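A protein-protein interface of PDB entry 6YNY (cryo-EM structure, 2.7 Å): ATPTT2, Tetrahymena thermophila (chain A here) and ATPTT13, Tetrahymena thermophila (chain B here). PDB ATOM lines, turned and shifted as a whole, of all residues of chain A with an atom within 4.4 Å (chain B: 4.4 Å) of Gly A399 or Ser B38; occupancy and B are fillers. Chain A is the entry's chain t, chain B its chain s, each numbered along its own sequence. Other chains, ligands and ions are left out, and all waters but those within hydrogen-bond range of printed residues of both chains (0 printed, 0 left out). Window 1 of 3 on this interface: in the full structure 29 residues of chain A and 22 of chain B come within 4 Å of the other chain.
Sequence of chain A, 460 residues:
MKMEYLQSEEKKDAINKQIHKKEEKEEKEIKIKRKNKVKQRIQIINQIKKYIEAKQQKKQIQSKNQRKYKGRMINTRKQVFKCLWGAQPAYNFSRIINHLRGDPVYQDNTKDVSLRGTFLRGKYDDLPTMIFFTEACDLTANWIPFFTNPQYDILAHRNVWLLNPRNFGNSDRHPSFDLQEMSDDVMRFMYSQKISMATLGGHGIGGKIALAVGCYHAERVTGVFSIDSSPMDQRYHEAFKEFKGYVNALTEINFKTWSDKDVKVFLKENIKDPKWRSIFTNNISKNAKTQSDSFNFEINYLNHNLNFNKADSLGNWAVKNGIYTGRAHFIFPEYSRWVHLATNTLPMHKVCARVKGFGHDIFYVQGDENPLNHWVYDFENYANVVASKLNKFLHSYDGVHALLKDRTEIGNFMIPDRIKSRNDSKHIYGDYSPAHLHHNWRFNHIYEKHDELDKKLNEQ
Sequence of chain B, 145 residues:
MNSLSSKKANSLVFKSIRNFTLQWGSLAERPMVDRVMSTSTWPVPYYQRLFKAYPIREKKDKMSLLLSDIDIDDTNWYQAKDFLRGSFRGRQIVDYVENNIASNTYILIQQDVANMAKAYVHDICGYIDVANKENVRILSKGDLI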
ATOM      1  N   THR A 222      11.460  17.565  14.509  1.00  0.00           N
ATOM      2  CA  THR A 222      10.630  18.741  14.727  1.00  0.00           C
ATOM      3  C   THR A 222      10.932  19.836  13.716  1.00  0.00           C
ATOM      4  O   THR A 222      10.018  20.525  13.251  1.00  0.00           O
ATOM      5  CB  THR A 222      10.831  19.262  16.148  1.00  0.00           C
ATOM      6  OG1 THR A 222      12.201  19.627  16.336  1.00  0.00           O
ATOM      7  CG2 THR A 222      10.455  18.202  17.151  1.00  0.00           C
ATOM      8  N   TYR A 397       9.178  28.754  15.925  1.00  0.00           N
ATOM      9  CA  TYR A 397       8.822  28.042  14.705  1.00  0.00           C
ATOM     10  C   TYR A 397       9.084  26.548  14.742  1.00  0.00           C
ATOM     11  O   TYR A 397       8.343  25.794  14.111  1.00  0.00           O
ATOM     12  CB  TYR A 397       9.568  28.631  13.506  1.00  0.00           C
ATOM     13  CG  TYR A 397       9.297  30.092  13.289  1.00  0.00           C
ATOM     14  CD1 TYR A 397       8.100  30.517  12.740  1.00  0.00           C
ATOM     15  CD2 TYR A 397      10.238  31.046  13.625  1.00  0.00           C
ATOM     16  CE1 TYR A 397       7.848  31.848  12.540  1.00  0.00           C
ATOM     17  CE2 TYR A 397       9.994  32.380  13.429  1.00  0.00           C
ATOM     18  CZ  TYR A 397       8.798  32.777  12.884  1.00  0.00           C
ATOM     19  OH  TYR A 397       8.549  34.111  12.687  1.00  0.00           O
ATOM     20  N   ASP A 398      10.105  26.094  15.457  1.00  0.00           N
ATOM     21  CA  ASP A 398      10.431  24.677  15.444  1.00  0.00           C
ATOM     22  C   ASP A 398       9.415  23.886  16.255  1.00  0.00           C
ATOM     23  O   ASP A 398       9.007  24.293  17.345  1.00  0.00           O
ATOM     24  CB  ASP A 398      11.833  24.447  15.995  1.00  0.00           C
ATOM     25  CG  ASP A 398      12.234  22.994  15.971  1.00  0.00           C
ATOM     26  OD1 ASP A 398      11.554  22.197  15.298  1.00  0.00           O
ATOM     27  OD2 ASP A 398      13.222  22.645  16.646  1.00  0.00           O
ATOM     28  N   GLY A 399       9.015  22.741  15.711  1.00  0.00           N
ATOM     29  CA  GLY A 399       8.051  21.885  16.368  1.00  0.00           C
ATOM     30  C   GLY A 399       6.675  22.494  16.466  1.00  0.00           C
ATOM     31  O   GLY A 399       5.942  22.208  17.416  1.00  0.00           O
ATOM     32  N   VAL A 400       6.304  23.323  15.500  1.00  0.00           N
ATOM     33  CA  VAL A 400       4.987  23.939  15.432  1.00  0.00           C
ATOM     34  C   VAL A 400       4.263  23.379  14.220  1.00  0.00           C
ATOM     35  O   VAL A 400       4.864  23.187  13.157  1.00  0.00           O
ATOM     36  CB  VAL A 400       5.082  25.473  15.358  1.00  0.00           C
ATOM     37  CG1 VAL A 400       3.714  26.075  15.201  1.00  0.00           C
ATOM     38  CG2 VAL A 400       5.737  26.016  16.594  1.00  0.00           C
ATOM     39  N   HIS A 401       2.975  23.106  14.387  1.00  0.00           N
ATOM     40  CA  HIS A 401       2.182  22.545  13.306  1.00  0.00           C
ATOM     41  C   HIS A 401       2.261  23.439  12.076  1.00  0.00           C
ATOM     42  O   HIS A 401       2.398  24.661  12.173  1.00  0.00           O
ATOM     43  CB  HIS A 401       0.733  22.375  13.751  1.00  0.00           C
ATOM     44  CG  HIS A 401      -0.087  21.528  12.832  1.00  0.00           C
ATOM     45  ND1 HIS A 401      -0.702  22.028  11.706  1.00  0.00           N
ATOM     46  CD2 HIS A 401      -0.400  20.213  12.879  1.00  0.00           C
ATOM     47  CE1 HIS A 401      -1.354  21.056  11.095  1.00  0.00           C
ATOM     48  NE2 HIS A 401      -1.187  19.944  11.787  1.00  0.00           N
ATOM     49  N   ARG A 407       4.392  29.651  17.529  1.00  0.00           N
ATOM     50  CA  ARG A 407       4.043  28.983  18.771  1.00  0.00           C
ATOM     51  C   ARG A 407       2.981  29.756  19.537  1.00  0.00           C
ATOM     52  O   ARG A 407       2.283  29.175  20.374  1.00  0.00           O
ATOM     53  CB  ARG A 407       5.294  28.803  19.622  1.00  0.00           C
ATOM     54  CG  ARG A 407       5.242  27.615  20.532  1.00  0.00           C
ATOM     55  CD  ARG A 407       6.594  27.313  21.126  1.00  0.00           C
ATOM     56  NE  ARG A 407       6.641  25.970  21.682  1.00  0.00           N
ATOM     57  CZ  ARG A 407       6.923  24.883  20.975  1.00  0.00           C
ATOM     58  NH1 ARG A 407       7.186  24.970  19.685  1.00  0.00           N
ATOM     59  NH2 ARG A 407       6.943  23.705  21.564  1.00  0.00           N
ATOM     60  N   ALA A 435      -2.699  18.593  18.073  1.00  0.00           N
ATOM     61  CA  ALA A 435      -2.000  18.163  19.272  1.00  0.00           C
ATOM     62  C   ALA A 435      -0.499  18.336  19.110  1.00  0.00           C
ATOM     63  O   ALA A 435       0.092  17.875  18.129  1.00  0.00           O
ATOM     64  CB  ALA A 435      -2.323  16.705  19.580  1.00  0.00           C
ATOM     65  N   HIS A 436       0.113  19.008  20.077  1.00  0.00           N
ATOM     66  CA  HIS A 436       1.558  19.125  20.182  1.00  0.00           C
ATOM     67  C   HIS A 436       1.992  18.355  21.419  1.00  0.00           C
ATOM     68  O   HIS A 436       1.528  18.645  22.526  1.00  0.00           O
ATOM     69  CB  HIS A 436       1.992  20.586  20.264  1.00  0.00           C
ATOM     70  CG  HIS A 436       1.692  21.381  19.035  1.00  0.00           C
ATOM     71  ND1 HIS A 436       0.409  21.618  18.594  1.00  0.00           N
ATOM     72  CD2 HIS A 436       2.512  22.000  18.154  1.00  0.00           C
ATOM     73  CE1 HIS A 436       0.452  22.346  17.494  1.00  0.00           C
ATOM     74  NE2 HIS A 436       1.716  22.591  17.205  1.00  0.00           N
ATOM     75  N   MET B  37       6.006  19.877  21.527  1.00  0.00           N
ATOM     76  CA  MET B  37       6.401  19.953  20.129  1.00  0.00           C
ATOM     77  C   MET B  37       5.445  19.140  19.264  1.00  0.00           C
ATOM     78  O   MET B  37       4.626  18.360  19.755  1.00  0.00           O
ATOM     79  CB  MET B  37       7.831  19.439  19.920  1.00  0.00           C
ATOM     80  CG  MET B  37       8.779  19.688  21.077  1.00  0.00           C
ATOM     81  SD  MET B  37       8.986  21.419  21.512  1.00  0.00           S
ATOM     82  CE  MET B  37       9.926  21.976  20.111  1.00  0.00           C
ATOM     83  N   SER B  38       5.566  19.338  17.953  1.00  0.00           N
ATOM     84  CA  SER B  38       4.824  18.566  16.966  1.00  0.00           C
ATOM     85  C   SER B  38       5.752  18.205  15.817  1.00  0.00           C
ATOM     86  O   SER B  38       6.784  18.843  15.599  1.00  0.00           O
ATOM     87  CB  SER B  38       3.616  19.333  16.426  1.00  0.00           C
ATOM     88  OG  SER B  38       2.994  18.625  15.372  1.00  0.00           O
ATOM     89  N   THR B  39       5.373  17.167  15.078  1.00  0.00           N
ATOM     90  CA  THR B  39       6.146  16.694  13.941  1.00  0.00           C
ATOM     91  C   THR B  39       5.247  16.576  12.720  1.00  0.00           C
ATOM     92  O   THR B  39       4.025  16.467  12.827  1.00  0.00           O
ATOM     93  CB  THR B  39       6.806  15.342  14.220  1.00  0.00           C
ATOM     94  OG1 THR B  39       5.809  14.377  14.563  1.00  0.00           O
ATOM     95  CG2 THR B  39       7.799  15.463  15.346  1.00  0.00           C
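OD1 of Asp A398 lies within hydrogen-bond range of OG1 of Thr A222. O of Thr A222 lies within hydrogen-bond range of N of Gly A399, 3.5 Å away. NH1 of Arg A407 lies within hydrogen-bond range of O of Asp A398. The backbone NH of His A401 is in hydrogen-bond range of a ring nitrogen (NE2) of His A436, 3.1 Å away.
SD of Met B37 sits at hydrogen-bond distance from NH2 of Arg A407, at 3.1 Å. The backbone NH of Ser B38 sits at hydrogen-bond distance from the backbone carbonyl oxygen of Gly A399 (2.9 Å).
Hydrophobic or aromatic side chains of chain A within 4 Å of the printed part of chain B: His A436. Hydrophobic or aromatic side chains of chain B that line the printed part of chain A: Met B37. Among the printed residues, no Asp or Glu carboxylate lies within 4 Å of a Lys or Arg side-chain nitrogen of the other chain.
Among the printed residues, merely in contact across the chains: Thr A222 with Ser B38 (3.9 Å), Asp A398 with Met B37 (3.7 Å), Gly A399 with Met B37 (3.6 Å), His A436 with Met B37 (3.1 Å) and His A436 with Ser B38 (3.4 Å).
Of the printed residues of chain B, Gly A399 touches Met B37 and Ser B38. Printed residues of chain B within 4 Å of Asp A398: Met B37 (3.7 Å). Printed residues of chain B within 4 Å of His A436: Met B37 (3.1 Å) and Ser B38 (3.4 Å). Printed residues of chain B within 4 Å of Arg A407: Met B37. Tyr A397 touches none of the printed residues of chain B. Val A400 touches none of the printed residues of chain B. The nearest residue of chain A that does not touch Ser B38 is Ala A435 (4.1 Å). The nearest printed residue of chain B that does not touch His A436 is Thr B39 (6.4 Å).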
